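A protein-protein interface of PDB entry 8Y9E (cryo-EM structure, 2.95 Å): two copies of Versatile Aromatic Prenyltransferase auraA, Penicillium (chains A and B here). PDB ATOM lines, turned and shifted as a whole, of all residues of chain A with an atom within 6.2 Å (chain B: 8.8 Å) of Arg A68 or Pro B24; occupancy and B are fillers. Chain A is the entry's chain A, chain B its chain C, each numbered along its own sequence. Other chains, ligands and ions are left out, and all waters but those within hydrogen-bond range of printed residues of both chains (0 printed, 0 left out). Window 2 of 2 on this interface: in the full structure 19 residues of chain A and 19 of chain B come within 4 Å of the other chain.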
ATOM      1  N   LEU A  63      19.428   2.565   0.468  1.00  0.00           N
ATOM      2  CA  LEU A  63      20.141   2.839  -0.772  1.00  0.00           C
ATOM      3  C   LEU A  63      21.627   2.538  -0.638  1.00  0.00           C
ATOM      4  O   LEU A  63      22.234   1.953  -1.543  1.00  0.00           O
ATOM      5  CB  LEU A  63      19.926   4.290  -1.178  1.00  0.00           C
ATOM      6  CG  LEU A  63      18.810   4.612  -2.162  1.00  0.00           C
ATOM      7  CD1 LEU A  63      19.162   4.077  -3.524  1.00  0.00           C
ATOM      8  CD2 LEU A  63      17.487   4.072  -1.677  1.00  0.00           C
ATOM      9  N   ASP A  64      22.233   2.933   0.479  1.00  0.00           N
ATOM     10  CA  ASP A  64      23.656   2.687   0.652  1.00  0.00           C
ATOM     11  C   ASP A  64      23.955   1.207   0.777  1.00  0.00           C
ATOM     12  O   ASP A  64      25.038   0.766   0.392  1.00  0.00           O
ATOM     13  CB  ASP A  64      24.181   3.431   1.870  1.00  0.00           C
ATOM     14  CG  ASP A  64      23.616   2.907   3.169  1.00  0.00           C
ATOM     15  OD1 ASP A  64      22.427   3.163   3.441  1.00  0.00           O
ATOM     16  OD2 ASP A  64      24.363   2.249   3.922  1.00  0.00           O
ATOM     17  N   VAL A  65      23.018   0.424   1.303  1.00  0.00           N
ATOM     18  CA  VAL A  65      23.227  -1.014   1.368  1.00  0.00           C
ATOM     19  C   VAL A  65      23.167  -1.619  -0.025  1.00  0.00           C
ATOM     20  O   VAL A  65      23.946  -2.517  -0.359  1.00  0.00           O
ATOM     21  CB  VAL A  65      22.204  -1.651   2.316  1.00  0.00           C
ATOM     22  CG1 VAL A  65      22.420  -3.107   2.399  1.00  0.00           C
ATOM     23  CG2 VAL A  65      22.339  -1.066   3.674  1.00  0.00           C
ATOM     24  N   GLN A  66      22.243  -1.145  -0.858  1.00  0.00           N
ATOM     25  CA  GLN A  66      22.259  -1.529  -2.262  1.00  0.00           C
ATOM     26  C   GLN A  66      23.610  -1.231  -2.885  1.00  0.00           C
ATOM     27  O   GLN A  66      24.183  -2.076  -3.577  1.00  0.00           O
ATOM     28  CB  GLN A  66      21.166  -0.799  -3.027  1.00  0.00           C
ATOM     29  CG  GLN A  66      19.783  -1.249  -2.728  1.00  0.00           C
ATOM     30  CD  GLN A  66      18.762  -0.540  -3.569  1.00  0.00           C
ATOM     31  OE1 GLN A  66      18.925  -0.398  -4.775  1.00  0.00           O
ATOM     32  NE2 GLN A  66      17.702  -0.081  -2.935  1.00  0.00           N
ATOM     33  N   TYR A  67      24.128  -0.028  -2.654  1.00  0.00           N
ATOM     34  CA  TYR A  67      25.427   0.337  -3.206  1.00  0.00           C
ATOM     35  C   TYR A  67      26.523  -0.591  -2.707  1.00  0.00           C
ATOM     36  O   TYR A  67      27.341  -1.081  -3.493  1.00  0.00           O
ATOM     37  CB  TYR A  67      25.749   1.778  -2.843  1.00  0.00           C
ATOM     38  CG  TYR A  67      25.304   2.791  -3.857  1.00  0.00           C
ATOM     39  CD1 TYR A  67      26.046   3.028  -4.992  1.00  0.00           C
ATOM     40  CD2 TYR A  67      24.145   3.519  -3.671  1.00  0.00           C
ATOM     41  CE1 TYR A  67      25.646   3.949  -5.915  1.00  0.00           C
ATOM     42  CE2 TYR A  67      23.741   4.443  -4.592  1.00  0.00           C
ATOM     43  CZ  TYR A  67      24.496   4.654  -5.711  1.00  0.00           C
ATOM     44  OH  TYR A  67      24.099   5.572  -6.643  1.00  0.00           O
ATOM     45  N   ARG A  68      26.553  -0.847  -1.400  1.00  0.00           N
ATOM     46  CA  ARG A  68      27.591  -1.692  -0.825  1.00  0.00           C
ATOM     47  C   ARG A  68      27.541  -3.094  -1.402  1.00  0.00           C
ATOM     48  O   ARG A  68      28.574  -3.649  -1.785  1.00  0.00           O
ATOM     49  CB  ARG A  68      27.443  -1.747   0.691  1.00  0.00           C
ATOM     50  CG  ARG A  68      27.766  -0.452   1.396  1.00  0.00           C
ATOM     51  CD  ARG A  68      28.181  -0.642   2.838  1.00  0.00           C
ATOM     52  NE  ARG A  68      29.153  -1.711   3.003  1.00  0.00           N
ATOM     53  CZ  ARG A  68      29.547  -2.185   4.177  1.00  0.00           C
ATOM     54  NH1 ARG A  68      29.050  -1.676   5.296  1.00  0.00           N
ATOM     55  NH2 ARG A  68      30.438  -3.164   4.229  1.00  0.00           N
ATOM     56  N   HIS A  69      26.353  -3.685  -1.470  1.00  0.00           N
ATOM     57  CA  HIS A  69      26.244  -5.061  -1.934  1.00  0.00           C
ATOM     58  C   HIS A  69      26.501  -5.168  -3.426  1.00  0.00           C
ATOM     59  O   HIS A  69      27.085  -6.151  -3.888  1.00  0.00           O
ATOM     60  CB  HIS A  69      24.877  -5.615  -1.585  1.00  0.00           C
ATOM     61  CG  HIS A  69      24.712  -5.911  -0.134  1.00  0.00           C
ATOM     62  ND1 HIS A  69      25.769  -6.263   0.673  1.00  0.00           N
ATOM     63  CD2 HIS A  69      23.620  -5.895   0.659  1.00  0.00           C
ATOM     64  CE1 HIS A  69      25.333  -6.459   1.902  1.00  0.00           C
ATOM     65  NE2 HIS A  69      24.032  -6.241   1.920  1.00  0.00           N
ATOM     66  N   LEU A  70      26.081  -4.173  -4.199  1.00  0.00           N
ATOM     67  CA  LEU A  70      26.373  -4.191  -5.620  1.00  0.00           C
ATOM     68  C   LEU A  70      27.857  -4.011  -5.876  1.00  0.00           C
ATOM     69  O   LEU A  70      28.399  -4.601  -6.812  1.00  0.00           O
ATOM     70  CB  LEU A  70      25.557  -3.114  -6.318  1.00  0.00           C
ATOM     71  CG  LEU A  70      24.058  -3.374  -6.311  1.00  0.00           C
ATOM     72  CD1 LEU A  70      23.299  -2.168  -6.717  1.00  0.00           C
ATOM     73  CD2 LEU A  70      23.736  -4.492  -7.227  1.00  0.00           C
ATOM     74  N   LEU A  71      28.544  -3.252  -5.031  1.00  0.00           N
ATOM     75  CA  LEU A  71      29.985  -3.123  -5.171  1.00  0.00           C
ATOM     76  C   LEU A  71      30.711  -4.383  -4.731  1.00  0.00           C
ATOM     77  O   LEU A  71      31.734  -4.745  -5.319  1.00  0.00           O
ATOM     78  CB  LEU A  71      30.464  -1.923  -4.369  1.00  0.00           C
ATOM     79  CG  LEU A  71      30.170  -0.574  -5.001  1.00  0.00           C
ATOM     80  CD1 LEU A  71      30.121   0.474  -3.946  1.00  0.00           C
ATOM     81  CD2 LEU A  71      31.212  -0.256  -6.020  1.00  0.00           C
ATOM     82  N   VAL A  72      30.201  -5.055  -3.702  1.00  0.00           N
ATOM     83  CA  VAL A  72      30.708  -6.372  -3.334  1.00  0.00           C
ATOM     84  C   VAL A  72      30.575  -7.330  -4.507  1.00  0.00           C
ATOM     85  O   VAL A  72      31.525  -8.026  -4.877  1.00  0.00           O
ATOM     86  CB  VAL A  72      29.965  -6.887  -2.090  1.00  0.00           C
ATOM     87  CG1 VAL A  72      30.271  -8.313  -1.840  1.00  0.00           C
ATOM     88  CG2 VAL A  72      30.344  -6.085  -0.888  1.00  0.00           C
ATOM     89  N   LEU A  73      29.384  -7.389  -5.098  1.00  0.00           N
ATOM     90  CA  LEU A  73      29.167  -8.198  -6.288  1.00  0.00           C
ATOM     91  C   LEU A  73      30.134  -7.816  -7.401  1.00  0.00           C
ATOM     92  O   LEU A  73      30.640  -8.683  -8.117  1.00  0.00           O
ATOM     93  CB  LEU A  73      27.715  -8.043  -6.734  1.00  0.00           C
ATOM     94  CG  LEU A  73      27.257  -8.457  -8.123  1.00  0.00           C
ATOM     95  CD1 LEU A  73      27.042  -9.923  -8.190  1.00  0.00           C
ATOM     96  CD2 LEU A  73      25.973  -7.776  -8.439  1.00  0.00           C
ATOM     97  N   LEU A 150      37.252  -6.960   2.156  1.00  0.00           N
ATOM     98  CA  LEU A 150      36.244  -5.911   2.169  1.00  0.00           C
ATOM     99  C   LEU A 150      35.607  -5.752   3.536  1.00  0.00           C
ATOM    100  O   LEU A 150      34.994  -4.715   3.804  1.00  0.00           O
ATOM    101  CB  LEU A 150      35.159  -6.198   1.138  1.00  0.00           C
ATOM    102  CG  LEU A 150      35.605  -6.405  -0.305  1.00  0.00           C
ATOM    103  CD1 LEU A 150      34.445  -6.291  -1.231  1.00  0.00           C
ATOM    104  CD2 LEU A 150      36.654  -5.418  -0.684  1.00  0.00           C
ATOM    105  N   GLN A 151      35.727  -6.752   4.391  1.00  0.00           N
ATOM    106  CA  GLN A 151      35.247  -6.668   5.768  1.00  0.00           C
ATOM    107  C   GLN A 151      36.145  -7.555   6.613  1.00  0.00           C
ATOM    108  O   GLN A 151      35.867  -8.750   6.792  1.00  0.00           O
ATOM    109  CB  GLN A 151      33.787  -7.089   5.896  1.00  0.00           C
ATOM    110  CG  GLN A 151      33.439  -8.334   5.135  1.00  0.00           C
ATOM    111  CD  GLN A 151      31.960  -8.601   5.116  1.00  0.00           C
ATOM    112  OE1 GLN A 151      31.154  -7.728   5.432  1.00  0.00           O
ATOM    113  NE2 GLN A 151      31.589  -9.820   4.750  1.00  0.00           N
ATOM    114  N   SER A 199      21.998  -5.095   6.850  1.00  0.00           N
ATOM    115  CA  SER A 199      22.996  -4.361   7.608  1.00  0.00           C
ATOM    116  C   SER A 199      24.285  -4.163   6.828  1.00  0.00           C
ATOM    117  O   SER A 199      25.314  -3.828   7.422  1.00  0.00           O
ATOM    118  CB  SER A 199      23.281  -5.085   8.920  1.00  0.00           C
ATOM    119  OG  SER A 199      22.121  -5.133   9.728  1.00  0.00           O
ATOM    120  N   ALA A 200      24.251  -4.380   5.518  1.00  0.00           N
ATOM    121  CA  ALA A 200      25.385  -4.244   4.614  1.00  0.00           C
ATOM    122  C   ALA A 200      26.440  -5.314   4.825  1.00  0.00           C
ATOM    123  O   ALA A 200      27.424  -5.359   4.079  1.00  0.00           O
ATOM    124  CB  ALA A 200      26.038  -2.869   4.732  1.00  0.00           C
ATOM    125  N   ALA A 201      26.268  -6.180   5.814  1.00  0.00           N
ATOM    126  CA  ALA A 201      27.205  -7.258   6.073  1.00  0.00           C
ATOM    127  C   ALA A 201      26.902  -8.435   5.161  1.00  0.00           C
ATOM    128  O   ALA A 201      25.780  -8.947   5.151  1.00  0.00           O
ATOM    129  CB  ALA A 201      27.130  -7.691   7.532  1.00  0.00           C
ATOM    130  N   SER B  23      31.032  -0.345  10.796  1.00  0.00           N
ATOM    131  CA  SER B  23      30.702   0.455   9.584  1.00  0.00           C
ATOM    132  C   SER B  23      31.938   1.075   8.945  1.00  0.00           C
ATOM    133  O   SER B  23      32.565   1.951   9.538  1.00  0.00           O
ATOM    134  CB  SER B  23      29.719   1.569   9.934  1.00  0.00           C
ATOM    135  OG  SER B  23      30.355   2.573  10.707  1.00  0.00           O
ATOM    136  N   PRO B  24      32.294   0.630   7.745  1.00  0.00           N
ATOM    137  CA  PRO B  24      33.227   1.408   6.935  1.00  0.00           C
ATOM    138  C   PRO B  24      32.521   2.612   6.345  1.00  0.00           C
ATOM    139  O   PRO B  24      31.339   2.569   6.000  1.00  0.00           O
ATOM    140  CB  PRO B  24      33.671   0.435   5.839  1.00  0.00           C
ATOM    141  CG  PRO B  24      33.116  -0.876   6.203  1.00  0.00           C
ATOM    142  CD  PRO B  24      31.934  -0.622   7.073  1.00  0.00           C
ATOM    143  N   SER B  25      33.252   3.685   6.241  1.00  0.00           N
ATOM    144  CA  SER B  25      32.667   4.864   5.639  1.00  0.00           C
ATOM    145  C   SER B  25      32.910   4.847   4.140  1.00  0.00           C
ATOM    146  O   SER B  25      33.871   4.240   3.659  1.00  0.00           O
ATOM    147  CB  SER B  25      33.254   6.116   6.269  1.00  0.00           C
ATOM    148  OG  SER B  25      33.026   6.128   7.667  1.00  0.00           O
ATOM    149  N   PRO B  26      32.044   5.501   3.371  1.00  0.00           N
ATOM    150  CA  PRO B  26      32.053   5.295   1.917  1.00  0.00           C
ATOM    151  C   PRO B  26      33.414   5.409   1.262  1.00  0.00           C
ATOM    152  O   PRO B  26      33.698   4.661   0.324  1.00  0.00           O
ATOM    153  CB  PRO B  26      31.104   6.382   1.426  1.00  0.00           C
ATOM    154  CG  PRO B  26      30.188   6.602   2.537  1.00  0.00           C
ATOM    155  CD  PRO B  26      30.958   6.398   3.788  1.00  0.00           C
ATOM    156  N   TRP B  27      34.265   6.322   1.718  1.00  0.00           N
ATOM    157  CA  TRP B  27      35.552   6.501   1.062  1.00  0.00           C
ATOM    158  C   TRP B  27      36.451   5.289   1.266  1.00  0.00           C
ATOM    159  O   TRP B  27      37.093   4.824   0.319  1.00  0.00           O
ATOM    160  CB  TRP B  27      36.231   7.782   1.549  1.00  0.00           C
ATOM    161  CG  TRP B  27      36.162   8.079   3.011  1.00  0.00           C
ATOM    162  CD1 TRP B  27      37.135   7.864   3.930  1.00  0.00           C
ATOM    163  CD2 TRP B  27      35.078   8.685   3.711  1.00  0.00           C
ATOM    164  NE1 TRP B  27      36.722   8.281   5.162  1.00  0.00           N
ATOM    165  CE2 TRP B  27      35.459   8.790   5.056  1.00  0.00           C
ATOM    166  CE3 TRP B  27      33.816   9.140   3.333  1.00  0.00           C
ATOM    167  CZ2 TRP B  27      34.624   9.328   6.024  1.00  0.00           C
ATOM    168  CZ3 TRP B  27      32.991   9.670   4.296  1.00  0.00           C
ATOM    169  CH2 TRP B  27      33.396   9.760   5.624  1.00  0.00           C
ATOM    170  N   ASP B  28      36.481   4.742   2.478  1.00  0.00           N
ATOM    171  CA  ASP B  28      37.282   3.551   2.736  1.00  0.00           C
ATOM    172  C   ASP B  28      36.792   2.377   1.897  1.00  0.00           C
ATOM    173  O   ASP B  28      37.562   1.749   1.160  1.00  0.00           O
ATOM    174  CB  ASP B  28      37.229   3.215   4.225  1.00  0.00           C
ATOM    175  CG  ASP B  28      37.946   4.231   5.079  1.00  0.00           C
ATOM    176  OD1 ASP B  28      38.966   4.786   4.622  1.00  0.00           O
ATOM    177  OD2 ASP B  28      37.487   4.475   6.214  1.00  0.00           O
ATOM    178  N   PHE B  29      35.501   2.066   2.004  1.00  0.00           N
ATOM    179  CA  PHE B  29      34.940   0.933   1.282  1.00  0.00           C
ATOM    180  C   PHE B  29      35.138   1.080  -0.220  1.00  0.00           C
ATOM    181  O   PHE B  29      35.453   0.107  -0.915  1.00  0.00           O
ATOM    182  CB  PHE B  29      33.461   0.794   1.635  1.00  0.00           C
ATOM    183  CG  PHE B  29      32.777  -0.321   0.932  1.00  0.00           C
ATOM    184  CD1 PHE B  29      33.028  -1.626   1.277  1.00  0.00           C
ATOM    185  CD2 PHE B  29      31.876  -0.066  -0.073  1.00  0.00           C
ATOM    186  CE1 PHE B  29      32.404  -2.647   0.634  1.00  0.00           C
ATOM    187  CE2 PHE B  29      31.250  -1.089  -0.717  1.00  0.00           C
ATOM    188  CZ  PHE B  29      31.516  -2.382  -0.362  1.00  0.00           C
ATOM    189  N   LEU B  30      34.984   2.297  -0.736  1.00  0.00           N
ATOM    190  CA  LEU B  30      35.117   2.509  -2.168  1.00  0.00           C
ATOM    191  C   LEU B  30      36.562   2.378  -2.611  1.00  0.00           C
ATOM    192  O   LEU B  30      36.839   1.830  -3.681  1.00  0.00           O
ATOM    193  CB  LEU B  30      34.568   3.875  -2.544  1.00  0.00           C
ATOM    194  CG  LEU B  30      33.059   4.017  -2.603  1.00  0.00           C
ATOM    195  CD1 LEU B  30      32.707   5.443  -2.703  1.00  0.00           C
ATOM    196  CD2 LEU B  30      32.514   3.302  -3.773  1.00  0.00           C
ATOM    197  N   ARG B  32      38.525   0.423  -1.303  1.00  0.00           N
ATOM    198  CA  ARG B  32      38.802  -1.002  -1.224  1.00  0.00           C
ATOM    199  C   ARG B  32      38.270  -1.745  -2.441  1.00  0.00           C
ATOM    200  O   ARG B  32      38.967  -2.600  -2.998  1.00  0.00           O
ATOM    201  CB  ARG B  32      38.199  -1.576   0.055  1.00  0.00           C
ATOM    202  CG  ARG B  32      38.878  -1.102   1.316  1.00  0.00           C
ATOM    203  CD  ARG B  32      38.919  -2.165   2.367  1.00  0.00           C
ATOM    204  NE  ARG B  32      37.641  -2.298   3.051  1.00  0.00           N
ATOM    205  CZ  ARG B  32      37.344  -1.716   4.206  1.00  0.00           C
ATOM    206  NH1 ARG B  32      38.225  -0.945   4.820  1.00  0.00           N
ATOM    207  NH2 ARG B  32      36.152  -1.903   4.744  1.00  0.00           N
ATOM    208  N   VAL B  33      37.053  -1.431  -2.876  1.00  0.00           N
ATOM    209  CA  VAL B  33      36.435  -2.194  -3.952  1.00  0.00           C
ATOM    210  C   VAL B  33      36.704  -1.607  -5.336  1.00  0.00           C
ATOM    211  O   VAL B  33      36.722  -2.347  -6.322  1.00  0.00           O
ATOM    212  CB  VAL B  33      34.925  -2.318  -3.712  1.00  0.00           C
ATOM    213  CG1 VAL B  33      34.651  -2.769  -2.317  1.00  0.00           C
ATOM    214  CG2 VAL B  33      34.264  -1.029  -3.960  1.00  0.00           C
ATOM    215  N   LEU B  63      23.987   8.775   3.115  1.00  0.00           N
ATOM    216  CA  LEU B  63      25.066   7.863   2.762  1.00  0.00           C
ATOM    217  C   LEU B  63      25.121   7.616   1.262  1.00  0.00           C
ATOM    218  O   LEU B  63      26.205   7.599   0.665  1.00  0.00           O
ATOM    219  CB  LEU B  63      24.893   6.550   3.512  1.00  0.00           C
ATOM    220  CG  LEU B  63      25.636   6.360   4.829  1.00  0.00           C
ATOM    221  CD1 LEU B  63      27.113   6.244   4.566  1.00  0.00           C
ATOM    222  CD2 LEU B  63      25.328   7.481   5.791  1.00  0.00           C
ATOM    223  N   ASP B  64      23.965   7.416   0.633  1.00  0.00           N
ATOM    224  CA  ASP B  64      23.960   7.159  -0.800  1.00  0.00           C
ATOM    225  C   ASP B  64      24.408   8.373  -1.587  1.00  0.00           C
ATOM    226  O   ASP B  64      24.979   8.225  -2.668  1.00  0.00           O
ATOM    227  CB  ASP B  64      22.578   6.720  -1.257  1.00  0.00           C
ATOM    228  CG  ASP B  64      21.543   7.815  -1.135  1.00  0.00           C
ATOM    229  OD1 ASP B  64      21.142   8.124   0.003  1.00  0.00           O
ATOM    230  OD2 ASP B  64      21.123   8.356  -2.178  1.00  0.00           O
ATOM    231  N   GLN B  66      26.723  10.508  -0.486  1.00  0.00           N
ATOM    232  CA  GLN B  66      28.168  10.372  -0.379  1.00  0.00           C
ATOM    233  C   GLN B  66      28.695   9.406  -1.422  1.00  0.00           C
ATOM    234  O   GLN B  66      29.677   9.696  -2.110  1.00  0.00           O
ATOM    235  CB  GLN B  66      28.557   9.893   1.012  1.00  0.00           C
ATOM    236  CG  GLN B  66      28.386  10.896   2.093  1.00  0.00           C
ATOM    237  CD  GLN B  66      28.855  10.383   3.422  1.00  0.00           C
ATOM    238  OE1 GLN B  66      29.928   9.800   3.532  1.00  0.00           O
ATOM    239  NE2 GLN B  66      28.049  10.588   4.445  1.00  0.00           N
ATOM    240  N   TYR B  67      28.057   8.245  -1.547  1.00  0.00           N
ATOM    241  CA  TYR B  67      28.491   7.264  -2.532  1.00  0.00           C
ATOM    242  C   TYR B  67      28.422   7.827  -3.944  1.00  0.00           C
ATOM    243  O   TYR B  67      29.370   7.687  -4.724  1.00  0.00           O
ATOM    244  CB  TYR B  67      27.632   6.014  -2.421  1.00  0.00           C
ATOM    245  CG  TYR B  67      28.175   4.965  -1.493  1.00  0.00           C
ATOM    246  CD1 TYR B  67      29.172   4.108  -1.902  1.00  0.00           C
ATOM    247  CD2 TYR B  67      27.680   4.826  -0.213  1.00  0.00           C
ATOM    248  CE1 TYR B  67      29.667   3.153  -1.065  1.00  0.00           C
ATOM    249  CE2 TYR B  67      28.171   3.871   0.631  1.00  0.00           C
ATOM    250  CZ  TYR B  67      29.163   3.037   0.198  1.00  0.00           C
ATOM    251  OH  TYR B  67      29.669   2.081   1.035  1.00  0.00           O
ATOM    252  N   LEU B  71      31.659   8.615  -6.284  1.00  0.00           N
ATOM    253  CA  LEU B  71      31.804   7.921  -7.552  1.00  0.00           C
ATOM    254  C   LEU B  71      31.898   8.891  -8.719  1.00  0.00           C
ATOM    255  O   LEU B  71      32.623   8.630  -9.683  1.00  0.00           O
ATOM    256  CB  LEU B  71      30.635   6.967  -7.743  1.00  0.00           C
ATOM    257  CG  LEU B  71      30.705   5.698  -6.913  1.00  0.00           C
ATOM    258  CD1 LEU B  71      29.335   5.155  -6.709  1.00  0.00           C
ATOM    259  CD2 LEU B  71      31.579   4.697  -7.594  1.00  0.00           C
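The guanidinium group (NH2) of Arg B32 sits at hydrogen-bond distance from the backbone carbonyl oxygen (O) of Leu A150 (3.2 Å).
Among the printed residues, merely in contact across the chains: Leu A63 with Asp B64 (3.6 Å), Asp A64 with Leu B63 (3.6 Å), Tyr A67 with Leu B71 (3.96 Å), Arg A68 with Pro B24 (3.5 Å), Arg A68 with Phe B29 (3.5 Å), Arg A68 with Tyr B67 (3.2 Å), Leu A71 with Phe B29 (3.8 Å), Leu A71 with Leu B30 (3.7 Å), Leu A71 with Val B33 (3.8 Å), Leu A71 with Tyr B67 (3.96 Å), Val A72 with Phe B29 (3.9 Å) and Leu A150 with Val B33 (3.7 Å).
Of the printed residues of chain B, Asp A64 touches Leu B63 (3.6 Å).
Val A65 touches none of the printed residues of chain B.
Arg A68 touches three residues of chain B.
Ser B23 touches none of the printed residues of chain A.
Pro B24 touches just one residue of chain A: Arg A68 (3.5 Å).
Printed residues of chain A within 4 Å of Leu B30: Leu A71.
Of the printed residues of chain A, Asp B64 touches Leu A63 (3.6 Å).
The nearest residue of chain B that does not touch Arg A68 is Ser B23 (5.1 Å).
The nearest residue of chain A that does not touch Pro B24 is Leu A150 (4.9 Å).
Hydrophobic or aromatic side chains of chain B that line the printed part of chain A: Pro B24, Phe B29, Leu B30, Val B33, Leu B63, Tyr B67 and Leu B71.
Along chain B the printed residues that touch a printed residue of chain A span positions 24 to 71.
Leu A63 touches Asp B64, and with the chains exchanged Asp A64 touches Leu B63.
Tyr A67 touches Leu B71, and with the chains exchanged Leu A71 touches Tyr B67.
Positions printed for both chains: 63, 64, 66, 67 and 71.
Of the 13 pairs that touch across the chains among the printed residues, 4 have their exchanged pair printed and touching as well.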
